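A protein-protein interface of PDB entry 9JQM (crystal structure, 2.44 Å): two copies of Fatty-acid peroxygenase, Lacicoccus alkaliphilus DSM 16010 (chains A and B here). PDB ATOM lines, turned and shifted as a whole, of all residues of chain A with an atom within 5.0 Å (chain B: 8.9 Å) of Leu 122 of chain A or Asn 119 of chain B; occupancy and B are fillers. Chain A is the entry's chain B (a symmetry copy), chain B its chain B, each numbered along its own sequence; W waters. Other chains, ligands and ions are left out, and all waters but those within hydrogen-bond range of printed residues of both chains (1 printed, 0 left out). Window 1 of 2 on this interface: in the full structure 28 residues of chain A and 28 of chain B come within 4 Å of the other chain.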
ATOM      1  N   ARG A 118     -34.725 -28.135 -16.189  1.00  0.00           N
ATOM      2  CA  ARG A 118     -34.865 -27.361 -14.961  1.00  0.00           C
ATOM      3  C   ARG A 118     -33.501 -26.972 -14.384  1.00  0.00           C
ATOM      4  O   ARG A 118     -33.303 -25.835 -13.940  1.00  0.00           O
ATOM      5  CB  ARG A 118     -35.687 -28.142 -13.947  1.00  0.00           C
ATOM      6  CG  ARG A 118     -35.851 -27.386 -12.637  1.00  0.00           C
ATOM      7  CD  ARG A 118     -36.394 -28.311 -11.606  1.00  0.00           C
ATOM      8  NE  ARG A 118     -37.694 -28.808 -12.034  1.00  0.00           N
ATOM      9  CZ  ARG A 118     -38.044 -30.089 -12.067  1.00  0.00           C
ATOM     10  NH1 ARG A 118     -37.192 -31.047 -11.724  1.00  0.00           N
ATOM     11  NH2 ARG A 118     -39.282 -30.416 -12.450  1.00  0.00           N
ATOM     12  N   ASN A 119     -32.538 -27.893 -14.401  1.00  0.00           N
ATOM     13  CA  ASN A 119     -31.272 -27.608 -13.735  1.00  0.00           C
ATOM     14  C   ASN A 119     -30.420 -26.640 -14.556  1.00  0.00           C
ATOM     15  O   ASN A 119     -29.737 -25.776 -13.991  1.00  0.00           O
ATOM     16  CB  ASN A 119     -30.529 -28.921 -13.442  1.00  0.00           C
ATOM     17  CG  ASN A 119     -31.264 -29.787 -12.395  1.00  0.00           C
ATOM     18  N   HIS A 120     -30.473 -26.750 -15.892  1.00  0.00           N
ATOM     19  CA  HIS A 120     -29.724 -25.838 -16.758  1.00  0.00           C
ATOM     20  C   HIS A 120     -30.200 -24.390 -16.612  1.00  0.00           C
ATOM     21  O   HIS A 120     -29.378 -23.467 -16.556  1.00  0.00           O
ATOM     22  CB  HIS A 120     -29.849 -26.302 -18.200  1.00  0.00           C
ATOM     23  CG  HIS A 120     -28.728 -27.180 -18.647  1.00  0.00           C
ATOM     24  ND1 HIS A 120     -28.728 -28.543 -18.449  1.00  0.00           N
ATOM     25  CD2 HIS A 120     -27.560 -26.889 -19.268  1.00  0.00           C
ATOM     26  CE1 HIS A 120     -27.623 -29.058 -18.955  1.00  0.00           C
ATOM     27  NE2 HIS A 120     -26.894 -28.074 -19.453  1.00  0.00           N
ATOM     28  N   TRP A 121     -31.525 -24.176 -16.523  1.00  0.00           N
ATOM     29  CA  TRP A 121     -32.060 -22.842 -16.236  1.00  0.00           C
ATOM     30  C   TRP A 121     -31.646 -22.358 -14.846  1.00  0.00           C
ATOM     31  O   TRP A 121     -31.140 -21.238 -14.697  1.00  0.00           O
ATOM     32  CB  TRP A 121     -33.602 -22.822 -16.402  1.00  0.00           C
ATOM     33  CG  TRP A 121     -34.011 -22.656 -17.865  1.00  0.00           C
ATOM     34  CD1 TRP A 121     -34.771 -23.519 -18.616  1.00  0.00           C
ATOM     35  CD2 TRP A 121     -33.618 -21.592 -18.766  1.00  0.00           C
ATOM     36  NE1 TRP A 121     -34.885 -23.056 -19.914  1.00  0.00           N
ATOM     37  CE2 TRP A 121     -34.191 -21.878 -20.029  1.00  0.00           C
ATOM     38  CE3 TRP A 121     -32.837 -20.425 -18.627  1.00  0.00           C
ATOM     39  CZ2 TRP A 121     -34.009 -21.040 -21.141  1.00  0.00           C
ATOM     40  CZ3 TRP A 121     -32.659 -19.585 -19.744  1.00  0.00           C
ATOM     41  CH2 TRP A 121     -33.243 -19.906 -20.977  1.00  0.00           C
ATOM     42  N   LEU A 122     -31.866 -23.183 -13.810  1.00  0.00           N
ATOM     43  CA  LEU A 122     -31.441 -22.810 -12.461  1.00  0.00           C
ATOM     44  C   LEU A 122     -29.967 -22.402 -12.428  1.00  0.00           C
ATOM     45  O   LEU A 122     -29.609 -21.401 -11.794  1.00  0.00           O
ATOM     46  CB  LEU A 122     -31.701 -23.969 -11.495  1.00  0.00           C
ATOM     47  CG  LEU A 122     -33.181 -24.171 -11.175  1.00  0.00           C
ATOM     48  CD1 LEU A 122     -33.439 -25.479 -10.432  1.00  0.00           C
ATOM     49  CD2 LEU A 122     -33.723 -22.976 -10.393  1.00  0.00           C
ATOM     50  N   MET A 123     -29.105 -23.145 -13.143  1.00  0.00           N
ATOM     51  CA  MET A 123     -27.667 -22.862 -13.130  1.00  0.00           C
ATOM     52  C   MET A 123     -27.290 -21.647 -13.974  1.00  0.00           C
ATOM     53  O   MET A 123     -26.278 -20.989 -13.693  1.00  0.00           O
ATOM     54  CB  MET A 123     -26.891 -24.094 -13.587  1.00  0.00           C
ATOM     55  CG  MET A 123     -26.810 -25.133 -12.465  1.00  0.00           C
ATOM     56  SD  MET A 123     -25.525 -24.740 -11.241  1.00  0.00           S
ATOM     57  CE  MET A 123     -24.319 -23.924 -12.303  1.00  0.00           C
ATOM     58  N   ASN A 124     -28.095 -21.326 -14.990  1.00  0.00           N
ATOM     59  CA  ASN A 124     -27.871 -20.186 -15.867  1.00  0.00           C
ATOM     60  C   ASN A 124     -28.233 -18.852 -15.231  1.00  0.00           C
ATOM     61  O   ASN A 124     -27.931 -17.804 -15.815  1.00  0.00           O
ATOM     62  CB  ASN A 124     -28.678 -20.382 -17.147  1.00  0.00           C
ATOM     63  CG  ASN A 124     -28.026 -19.760 -18.345  1.00  0.00           C
ATOM     64  OD1 ASN A 124     -26.840 -19.976 -18.625  1.00  0.00           O
ATOM     65  ND2 ASN A 124     -28.807 -18.977 -19.084  1.00  0.00           N
ATOM     66  N   THR A 125     -28.844 -18.854 -14.046  1.00  0.00           N
ATOM     67  CA  THR A 125     -29.326 -17.598 -13.472  1.00  0.00           C
ATOM     68  C   THR A 125     -28.180 -16.632 -13.196  1.00  0.00           C
ATOM     69  O   THR A 125     -28.240 -15.457 -13.572  1.00  0.00           O
ATOM     70  CB  THR A 125     -30.113 -17.867 -12.200  1.00  0.00           C
ATOM     71  OG1 THR A 125     -31.208 -18.726 -12.516  1.00  0.00           O
ATOM     72  CG2 THR A 125     -30.634 -16.559 -11.609  1.00  0.00           C
ATOM     73  N   TYR A 383     -39.829 -21.554 -14.945  1.00  0.00           N
ATOM     74  CA  TYR A 383     -38.601 -20.861 -14.581  1.00  0.00           C
ATOM     75  C   TYR A 383     -38.754 -19.348 -14.742  1.00  0.00           C
ATOM     76  O   TYR A 383     -38.571 -18.592 -13.783  1.00  0.00           O
ATOM     77  CB  TYR A 383     -37.433 -21.387 -15.426  1.00  0.00           C
ATOM     78  CG  TYR A 383     -36.187 -20.570 -15.233  1.00  0.00           C
ATOM     79  CD1 TYR A 383     -35.433 -20.695 -14.056  1.00  0.00           C
ATOM     80  CD2 TYR A 383     -35.775 -19.640 -16.196  1.00  0.00           C
ATOM     81  CE1 TYR A 383     -34.298 -19.942 -13.850  1.00  0.00           C
ATOM     82  CE2 TYR A 383     -34.641 -18.874 -15.993  1.00  0.00           C
ATOM     83  CZ  TYR A 383     -33.901 -19.030 -14.814  1.00  0.00           C
ATOM     84  OH  TYR A 383     -32.759 -18.287 -14.593  1.00  0.00           O
ATOM     85  N   ARG A 387     -38.849 -18.182 -11.079  1.00  0.00           N
ATOM     86  CA  ARG A 387     -37.500 -18.169 -10.514  1.00  0.00           C
ATOM     87  C   ARG A 387     -36.769 -16.837 -10.654  1.00  0.00           C
ATOM     88  O   ARG A 387     -35.899 -16.532  -9.831  1.00  0.00           O
ATOM     89  CB  ARG A 387     -36.610 -19.236 -11.153  1.00  0.00           C
ATOM     90  CG  ARG A 387     -36.738 -20.575 -10.558  1.00  0.00           C
ATOM     91  CD  ARG A 387     -36.627 -20.544  -9.024  1.00  0.00           C
ATOM     92  NE  ARG A 387     -35.282 -20.476  -8.457  1.00  0.00           N
ATOM     93  CZ  ARG A 387     -34.897 -21.237  -7.433  1.00  0.00           C
ATOM     94  NH1 ARG A 387     -35.716 -22.130  -6.890  1.00  0.00           N
ATOM     95  NH2 ARG A 387     -33.660 -21.119  -6.952  1.00  0.00           N
ATOM     96  N   GLU A 419     -32.534 -13.621  -9.499  1.00  0.00           N
ATOM     97  CA  GLU A 419     -33.172 -14.810  -8.955  1.00  0.00           C
ATOM     98  C   GLU A 419     -34.176 -14.425  -7.881  1.00  0.00           C
ATOM     99  O   GLU A 419     -34.026 -13.410  -7.197  1.00  0.00           O
ATOM    100  CB  GLU A 419     -32.129 -15.766  -8.373  1.00  0.00           C
ATOM    101  CG  GLU A 419     -32.681 -17.126  -8.037  1.00  0.00           C
ATOM    102  CD  GLU A 419     -31.610 -18.199  -7.972  1.00  0.00           C
ATOM    103  OE1 GLU A 419     -30.428 -17.844  -7.765  1.00  0.00           O
ATOM    104  OE2 GLU A 419     -31.958 -19.400  -8.111  1.00  0.00           O
ATOM    105  N   GLN B 111     -33.316 -23.719   2.492  1.00  0.00           N
ATOM    106  CA  GLN B 111     -33.842 -24.443   1.340  1.00  0.00           C
ATOM    107  C   GLN B 111     -33.157 -23.978   0.066  1.00  0.00           C
ATOM    108  O   GLN B 111     -32.888 -24.778  -0.835  1.00  0.00           O
ATOM    109  CB  GLN B 111     -35.361 -24.269   1.247  1.00  0.00           C
ATOM    110  CG  GLN B 111     -36.015 -24.806  -0.040  1.00  0.00           C
ATOM    111  CD  GLN B 111     -35.985 -26.338  -0.145  1.00  0.00           C
ATOM    112  OE1 GLN B 111     -36.040 -27.064   0.865  1.00  0.00           O
ATOM    113  NE2 GLN B 111     -35.913 -26.835  -1.382  1.00  0.00           N
ATOM    114  N   TYR B 112     -32.879 -22.682  -0.022  1.00  0.00           N
ATOM    115  CA  TYR B 112     -31.979 -22.192  -1.050  1.00  0.00           C
ATOM    116  C   TYR B 112     -30.661 -22.960  -1.028  1.00  0.00           C
ATOM    117  O   TYR B 112     -30.210 -23.463  -2.068  1.00  0.00           O
ATOM    118  CB  TYR B 112     -31.739 -20.697  -0.866  1.00  0.00           C
ATOM    119  CG  TYR B 112     -31.047 -20.078  -2.064  1.00  0.00           C
ATOM    120  CD1 TYR B 112     -31.382 -20.458  -3.367  1.00  0.00           C
ATOM    121  CD2 TYR B 112     -30.053 -19.127  -1.897  1.00  0.00           C
ATOM    122  CE1 TYR B 112     -30.752 -19.881  -4.472  1.00  0.00           C
ATOM    123  CE2 TYR B 112     -29.421 -18.552  -2.985  1.00  0.00           C
ATOM    124  CZ  TYR B 112     -29.773 -18.924  -4.264  1.00  0.00           C
ATOM    125  OH  TYR B 112     -29.136 -18.330  -5.328  1.00  0.00           O
ATOM    126  N   LEU B 113     -30.036 -23.078   0.158  1.00  0.00           N
ATOM    127  CA  LEU B 113     -28.785 -23.828   0.262  1.00  0.00           C
ATOM    128  C   LEU B 113     -28.947 -25.265  -0.233  1.00  0.00           C
ATOM    129  O   LEU B 113     -28.070 -25.790  -0.931  1.00  0.00           O
ATOM    130  CB  LEU B 113     -28.273 -23.820   1.697  1.00  0.00           C
ATOM    131  CG  LEU B 113     -27.012 -24.678   1.877  1.00  0.00           C
ATOM    132  CD1 LEU B 113     -25.843 -24.111   1.049  1.00  0.00           C
ATOM    133  CD2 LEU B 113     -26.603 -24.811   3.324  1.00  0.00           C
ATOM    134  N   ARG B 114     -30.071 -25.908   0.090  1.00  0.00           N
ATOM    135  CA  ARG B 114     -30.281 -27.286  -0.343  1.00  0.00           C
ATOM    136  C   ARG B 114     -30.366 -27.382  -1.861  1.00  0.00           C
ATOM    137  O   ARG B 114     -29.782 -28.291  -2.475  1.00  0.00           O
ATOM    138  CB  ARG B 114     -31.555 -27.850   0.292  1.00  0.00           C
ATOM    139  CG  ARG B 114     -31.815 -29.284  -0.115  1.00  0.00           C
ATOM    140  CD  ARG B 114     -33.206 -29.778   0.245  1.00  0.00           C
ATOM    141  NE  ARG B 114     -33.708 -29.169   1.472  1.00  0.00           N
ATOM    142  CZ  ARG B 114     -33.480 -29.638   2.695  1.00  0.00           C
ATOM    143  NH1 ARG B 114     -32.716 -30.704   2.901  1.00  0.00           N
ATOM    144  NH2 ARG B 114     -34.040 -29.027   3.741  1.00  0.00           N
ATOM    145  N   GLU B 115     -31.096 -26.450  -2.480  1.00  0.00           N
ATOM    146  CA  GLU B 115     -31.248 -26.460  -3.931  1.00  0.00           C
ATOM    147  C   GLU B 115     -29.926 -26.180  -4.623  1.00  0.00           C
ATOM    148  O   GLU B 115     -29.598 -26.834  -5.626  1.00  0.00           O
ATOM    149  CB  GLU B 115     -32.310 -25.444  -4.347  1.00  0.00           C
ATOM    150  CG  GLU B 115     -33.712 -25.908  -3.964  1.00  0.00           C
ATOM    151  CD  GLU B 115     -34.773 -24.807  -4.007  1.00  0.00           C
ATOM    152  OE1 GLU B 115     -34.546 -23.727  -4.601  1.00  0.00           O
ATOM    153  OE2 GLU B 115     -35.847 -25.036  -3.410  1.00  0.00           O
ATOM    154  N   LEU B 116     -29.154 -25.216  -4.105  1.00  0.00           N
ATOM    155  CA  LEU B 116     -27.846 -24.923  -4.691  1.00  0.00           C
ATOM    156  C   LEU B 116     -26.965 -26.164  -4.708  1.00  0.00           C
ATOM    157  O   LEU B 116     -26.307 -26.460  -5.721  1.00  0.00           O
ATOM    158  CB  LEU B 116     -27.145 -23.814  -3.916  1.00  0.00           C
ATOM    159  CG  LEU B 116     -27.622 -22.380  -4.084  1.00  0.00           C
ATOM    160  CD1 LEU B 116     -26.880 -21.495  -3.068  1.00  0.00           C
ATOM    161  CD2 LEU B 116     -27.369 -21.933  -5.495  1.00  0.00           C
ATOM    162  N   THR B 117     -26.947 -26.908  -3.590  1.00  0.00           N
ATOM    163  CA  THR B 117     -26.095 -28.087  -3.509  1.00  0.00           C
ATOM    164  C   THR B 117     -26.556 -29.156  -4.482  1.00  0.00           C
ATOM    165  O   THR B 117     -25.736 -29.747  -5.201  1.00  0.00           O
ATOM    166  CB  THR B 117     -26.073 -28.626  -2.086  1.00  0.00           C
ATOM    167  OG1 THR B 117     -25.634 -27.586  -1.198  1.00  0.00           O
ATOM    168  CG2 THR B 117     -25.144 -29.842  -2.004  1.00  0.00           C
ATOM    169  N   ARG B 118     -27.862 -29.386  -4.558  1.00  0.00           N
ATOM    170  CA  ARG B 118     -28.355 -30.434  -5.441  1.00  0.00           C
ATOM    171  C   ARG B 118     -28.076 -30.109  -6.912  1.00  0.00           C
ATOM    172  O   ARG B 118     -27.666 -30.980  -7.687  1.00  0.00           O
ATOM    173  CB  ARG B 118     -29.841 -30.658  -5.202  1.00  0.00           C
ATOM    174  CG  ARG B 118     -30.413 -31.734  -6.112  1.00  0.00           C
ATOM    175  CD  ARG B 118     -31.899 -31.692  -6.041  1.00  0.00           C
ATOM    176  NE  ARG B 118     -32.328 -31.949  -4.673  1.00  0.00           N
ATOM    177  CZ  ARG B 118     -33.177 -31.189  -3.989  1.00  0.00           C
ATOM    178  NH1 ARG B 118     -33.693 -30.086  -4.514  1.00  0.00           N
ATOM    179  NH2 ARG B 118     -33.518 -31.550  -2.749  1.00  0.00           N
ATOM    180  N   ASN B 119     -28.270 -28.852  -7.313  1.00  0.00           N
ATOM    181  CA  ASN B 119     -28.151 -28.533  -8.731  1.00  0.00           C
ATOM    182  C   ASN B 119     -26.686 -28.494  -9.169  1.00  0.00           C
ATOM    183  O   ASN B 119     -26.356 -28.917 -10.284  1.00  0.00           O
ATOM    184  CB  ASN B 119     -28.877 -27.213  -9.032  1.00  0.00           C
ATOM    185  CG  ASN B 119     -30.407 -27.334  -8.850  1.00  0.00           C
ATOM    186  N   HIS B 120     -25.791 -28.017  -8.290  1.00  0.00           N
ATOM    187  CA  HIS B 120     -24.363 -27.981  -8.607  1.00  0.00           C
ATOM    188  C   HIS B 120     -23.786 -29.385  -8.808  1.00  0.00           C
ATOM    189  O   HIS B 120     -23.000 -29.608  -9.738  1.00  0.00           O
ATOM    190  CB  HIS B 120     -23.623 -27.250  -7.499  1.00  0.00           C
ATOM    191  CG  HIS B 120     -23.421 -25.796  -7.770  1.00  0.00           C
ATOM    192  ND1 HIS B 120     -24.365 -24.844  -7.456  1.00  0.00           N
ATOM    193  CD2 HIS B 120     -22.391 -25.130  -8.343  1.00  0.00           C
ATOM    194  CE1 HIS B 120     -23.914 -23.652  -7.795  1.00  0.00           C
ATOM    195  NE2 HIS B 120     -22.719 -23.797  -8.342  1.00  0.00           N
ATOM    196  N   TRP B 121     -24.185 -30.349  -7.960  1.00  0.00           N
ATOM    197  CA  TRP B 121     -23.799 -31.749  -8.166  1.00  0.00           C
ATOM    198  C   TRP B 121     -24.389 -32.309  -9.461  1.00  0.00           C
ATOM    199  O   TRP B 121     -23.665 -32.893 -10.278  1.00  0.00           O
ATOM    200  CB  TRP B 121     -24.200 -32.615  -6.944  1.00  0.00           C
ATOM    201  CG  TRP B 121     -23.174 -32.512  -5.816  1.00  0.00           C
ATOM    202  CD1 TRP B 121     -23.395 -32.076  -4.532  1.00  0.00           C
ATOM    203  CD2 TRP B 121     -21.755 -32.787  -5.900  1.00  0.00           C
ATOM    204  NE1 TRP B 121     -22.213 -32.074  -3.815  1.00  0.00           N
ATOM    205  CE2 TRP B 121     -21.197 -32.507  -4.629  1.00  0.00           C
ATOM    206  CE3 TRP B 121     -20.901 -33.243  -6.928  1.00  0.00           C
ATOM    207  CZ2 TRP B 121     -19.829 -32.671  -4.359  1.00  0.00           C
ATOM    208  CZ3 TRP B 121     -19.528 -33.408  -6.652  1.00  0.00           C
ATOM    209  CH2 TRP B 121     -19.017 -33.118  -5.379  1.00  0.00           C
ATOM    210  N   LEU B 122     -25.707 -32.154  -9.662  1.00  0.00           N
ATOM    211  CA  LEU B 122     -26.328 -32.612 -10.903  1.00  0.00           C
ATOM    212  C   LEU B 122     -25.601 -32.062 -12.132  1.00  0.00           C
ATOM    213  O   LEU B 122     -25.354 -32.800 -13.095  1.00  0.00           O
ATOM    214  CB  LEU B 122     -27.805 -32.210 -10.926  1.00  0.00           C
ATOM    215  CG  LEU B 122     -28.670 -33.029  -9.971  1.00  0.00           C
ATOM    216  CD1 LEU B 122     -30.071 -32.443  -9.814  1.00  0.00           C
ATOM    217  CD2 LEU B 122     -28.731 -34.486 -10.426  1.00  0.00           C
ATOM    218  N   MET B 123     -25.214 -30.775 -12.095  1.00  0.00           N
ATOM    219  CA  MET B 123     -24.559 -30.148 -13.246  1.00  0.00           C
ATOM    220  C   MET B 123     -23.097 -30.562 -13.400  1.00  0.00           C
ATOM    221  O   MET B 123     -22.566 -30.548 -14.521  1.00  0.00           O
ATOM    222  CB  MET B 123     -24.677 -28.628 -13.146  1.00  0.00           C
ATOM    223  CG  MET B 123     -26.079 -28.166 -13.550  1.00  0.00           C
ATOM    224  SD  MET B 123     -26.299 -28.095 -15.353  1.00  0.00           S
ATOM    225  CE  MET B 123     -24.625 -27.655 -15.856  1.00  0.00           C
ATOM    226  N   ASN B 124     -22.445 -30.950 -12.301  1.00  0.00           N
ATOM    227  CA  ASN B 124     -21.057 -31.387 -12.300  1.00  0.00           C
ATOM    228  C   ASN B 124     -20.865 -32.795 -12.844  1.00  0.00           C
ATOM    229  O   ASN B 124     -19.719 -33.213 -13.046  1.00  0.00           O
ATOM    230  CB  ASN B 124     -20.515 -31.308 -10.877  1.00  0.00           C
ATOM    231  CG  ASN B 124     -19.047 -31.005 -10.830  1.00  0.00           C
ATOM    232  OD1 ASN B 124     -18.558 -30.062 -11.461  1.00  0.00           O
ATOM    233  ND2 ASN B 124     -18.318 -31.812 -10.063  1.00  0.00           N
ATOM    234  N   THR B 125     -21.946 -33.531 -13.110  1.00  0.00           N
ATOM    235  CA  THR B 125     -21.797 -34.931 -13.503  1.00  0.00           C
ATOM    236  C   THR B 125     -21.035 -35.067 -14.816  1.00  0.00           C
ATOM    237  O   THR B 125     -20.091 -35.857 -14.920  1.00  0.00           O
ATOM    238  CB  THR B 125     -23.159 -35.597 -13.607  1.00  0.00           C
ATOM    239  OG1 THR B 125     -23.812 -35.499 -12.342  1.00  0.00           O
ATOM    240  CG2 THR B 125     -23.006 -37.066 -13.999  1.00  0.00           C
ATOM    241  N   LEU B 143     -16.565 -27.367  -5.885  1.00  0.00           N
ATOM    242  CA  LEU B 143     -18.023 -27.294  -5.913  1.00  0.00           C
ATOM    243  C   LEU B 143     -18.570 -26.460  -4.755  1.00  0.00           C
ATOM    244  O   LEU B 143     -19.402 -25.557  -4.958  1.00  0.00           O
ATOM    245  CB  LEU B 143     -18.628 -28.686  -5.892  1.00  0.00           C
ATOM    246  CG  LEU B 143     -20.113 -28.602  -6.251  1.00  0.00           C
ATOM    247  CD1 LEU B 143     -20.454 -29.643  -7.310  1.00  0.00           C
ATOM    248  CD2 LEU B 143     -21.008 -28.750  -4.991  1.00  0.00           C
ATOM    249  N   VAL B 147     -20.952 -22.960  -4.456  1.00  0.00           N
ATOM    250  CA  VAL B 147     -22.205 -22.958  -3.708  1.00  0.00           C
ATOM    251  C   VAL B 147     -22.169 -21.909  -2.606  1.00  0.00           C
ATOM    252  O   VAL B 147     -23.134 -21.160  -2.410  1.00  0.00           O
ATOM    253  CB  VAL B 147     -22.481 -24.352  -3.129  1.00  0.00           C
ATOM    254  CG1 VAL B 147     -23.512 -24.259  -2.025  1.00  0.00           C
ATOM    255  CG2 VAL B 147     -22.897 -25.328  -4.222  1.00  0.00           C
ATOM    256  N   ARG B 150     -22.173 -18.188  -3.827  1.00  0.00           N
ATOM    257  CA  ARG B 150     -23.539 -17.870  -4.230  1.00  0.00           C
ATOM    258  C   ARG B 150     -24.445 -17.693  -3.018  1.00  0.00           C
ATOM    259  O   ARG B 150     -25.152 -16.684  -2.894  1.00  0.00           O
ATOM    260  CB  ARG B 150     -24.085 -18.966  -5.154  1.00  0.00           C
ATOM    261  CG  ARG B 150     -25.494 -18.705  -5.633  1.00  0.00           C
ATOM    262  CD  ARG B 150     -25.559 -17.377  -6.351  1.00  0.00           C
ATOM    263  NE  ARG B 150     -26.794 -17.202  -7.110  1.00  0.00           N
ATOM    264  CZ  ARG B 150     -27.085 -16.124  -7.831  1.00  0.00           C
ATOM    265  NH1 ARG B 150     -26.226 -15.126  -7.966  1.00  0.00           N
ATOM    266  NH2 ARG B 150     -28.271 -16.039  -8.415  1.00  0.00           N
ATOM    267  N   GLU B 379     -27.652 -33.831   0.982  1.00  0.00           N
ATOM    268  CA  GLU B 379     -27.706 -33.686  -0.469  1.00  0.00           C
ATOM    269  C   GLU B 379     -26.522 -34.369  -1.138  1.00  0.00           C
ATOM    270  O   GLU B 379     -26.693 -35.126  -2.103  1.00  0.00           O
ATOM    271  CB  GLU B 379     -27.759 -32.203  -0.845  1.00  0.00           C
ATOM    272  CG  GLU B 379     -29.132 -31.563  -0.645  1.00  0.00           C
ATOM    273  CD  GLU B 379     -30.246 -32.405  -1.250  1.00  0.00           C
ATOM    274  OE1 GLU B 379     -30.152 -32.742  -2.458  1.00  0.00           O
ATOM    275  OE2 GLU B 379     -31.203 -32.737  -0.527  1.00  0.00           O
ATOM    276  N   TYR B 383     -26.684 -37.675  -3.669  1.00  0.00           N
ATOM    277  CA  TYR B 383     -26.118 -37.588  -5.008  1.00  0.00           C
ATOM    278  C   TYR B 383     -25.165 -38.752  -5.280  1.00  0.00           C
ATOM    279  O   TYR B 383     -25.361 -39.514  -6.233  1.00  0.00           O
ATOM    280  CB  TYR B 383     -25.403 -36.242  -5.186  1.00  0.00           C
ATOM    281  CG  TYR B 383     -24.632 -36.181  -6.475  1.00  0.00           C
ATOM    282  CD1 TYR B 383     -25.305 -36.020  -7.695  1.00  0.00           C
ATOM    283  CD2 TYR B 383     -23.239 -36.324  -6.491  1.00  0.00           C
ATOM    284  CE1 TYR B 383     -24.620 -35.981  -8.889  1.00  0.00           C
ATOM    285  CE2 TYR B 383     -22.545 -36.295  -7.688  1.00  0.00           C
ATOM    286  CZ  TYR B 383     -23.243 -36.120  -8.890  1.00  0.00           C
ATOM    287  OH  TYR B 383     -22.572 -36.074 -10.095  1.00  0.00           O
HETATM  288  O   HOH W   1     -28.236 -19.853  -8.670  1.00  0.00           O
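The side-chain carboxylate (OE1) of Glu 419 of chain A is in hydrogen-bond range of the side-chain hydroxyl (OH) of Tyr 112 of chain B, at 2.8 Å. The side-chain carboxylate (OE1) of Glu 115 of chain B lies within salt-bridge range of the guanidinium group (NH1) of Arg 387 of chain A (3.0 Å). The side-chain carboxylate of Glu 419 of chain A is in salt-bridge range of the guanidinium group of Arg 150 of chain B, at 2.9 Å.
The side-chain carboxylate (OE2) of Glu 115 of chain B is in hydrogen-bond range of the side-chain amide nitrogen (NE2) of Gln 111 of chain B, 2.7 Å away. NE of Arg 150 of chain B is in hydrogen-bond range of OH of Tyr 112 of chain B, at 3.2 Å. The backbone carbonyl oxygen (O) of Leu 116 of chain B lies within hydrogen-bond range of a ring nitrogen (ND1) of His 120 of chain B (3.1 Å). The side-chain hydroxyl (OG1) of Thr 125 of chain B lies within hydrogen-bond range of the backbone carbonyl oxygen (O) of Leu 122 of chain B (3.2 Å). The backbone carbonyl oxygen of Leu 122 of chain A lies within hydrogen-bond range of the side-chain hydroxyl of Thr 125 of chain A (3.2 Å). The side-chain carboxylate (OE2) of Glu 419 of chain A is in salt-bridge range of the guanidinium group (NH2) of Arg 387 of chain A.
Asn 119 of chain A touches Leu 122 of chain B (CG to CD1, 3.9 Å). SD of Met 123 of chain B touches CE1 of His 120 of chain A (3.96 Å). Leu 122 of chain A touches Asn 119 of chain B. His 120 of chain B touches Met 123 of chain A (CE1 to SD, 3.96 Å). CG of Met 123 of chain A touches CG of Met 123 of chain B (3.3 Å).
Of chain B, only Asn 119 comes within 4 Å of Leu 122 of chain A. Of chain A, only Leu 122 (3.9 Å) comes within 4 Å of Asn 119 of chain B. Printed residues of chain A within 4 Å of Arg 150 of chain B: Glu 419. Of the printed residues of chain B, His 120 of chain A touches Met 123 (3.96 Å). Printed residues of chain A within 4 Å of Glu 115 of chain B: Arg 387. Printed residues of chain B within 4 Å of Met 123 of chain A: His 120 and Met 123. The nearest residue of chain B that does not touch Leu 122 of chain A is Glu 115 of chain B (5.9 Å). The nearest printed residue of chain B that does not touch Met 123 of chain A is Asn 119 of chain B (4.4 Å).
Hydrophobic or aromatic side chains of chain A that line the printed part of chain B: His 120, Leu 122 and Met 123. Of the 20 printed residues of chain B, 7 touch a printed residue of chain A. Hydrophobic or aromatic side chains of chain B that line the printed part of chain A: Tyr 112, His 120, Leu 122 and Met 123. Among the printed residues, Asp or Glu carboxylates within 4 Å of a Lys or Arg side-chain nitrogen of the other chain: Arg 387 of chain A with Glu 115 of chain B and Glu 419 of chain A with Arg 150 of chain B.
Asn 119 of chain A touches Leu 122 of chain B, and with the chains exchanged Leu 122 of chain A touches Asn 119 of chain B. His 120 of chain A touches Met 123 of chain B, and with the chains exchanged Met 123 of chain A touches His 120 of chain B. Met 123 of chain A touches its own counterpart, Met 123 of chain B. Positions printed for both chains: 118, 119, 120, 121, 122, 123, 124, 125 and 383. Of the 8 pairs that touch across the chains among the printed residues, 5 have their exchanged pair printed and touching as well.
Water W1 lies within hydrogen-bond range of OE1 of Glu 419 of chain A (3.1 Å) and NE of Arg 150 of chain B (3.4 Å).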
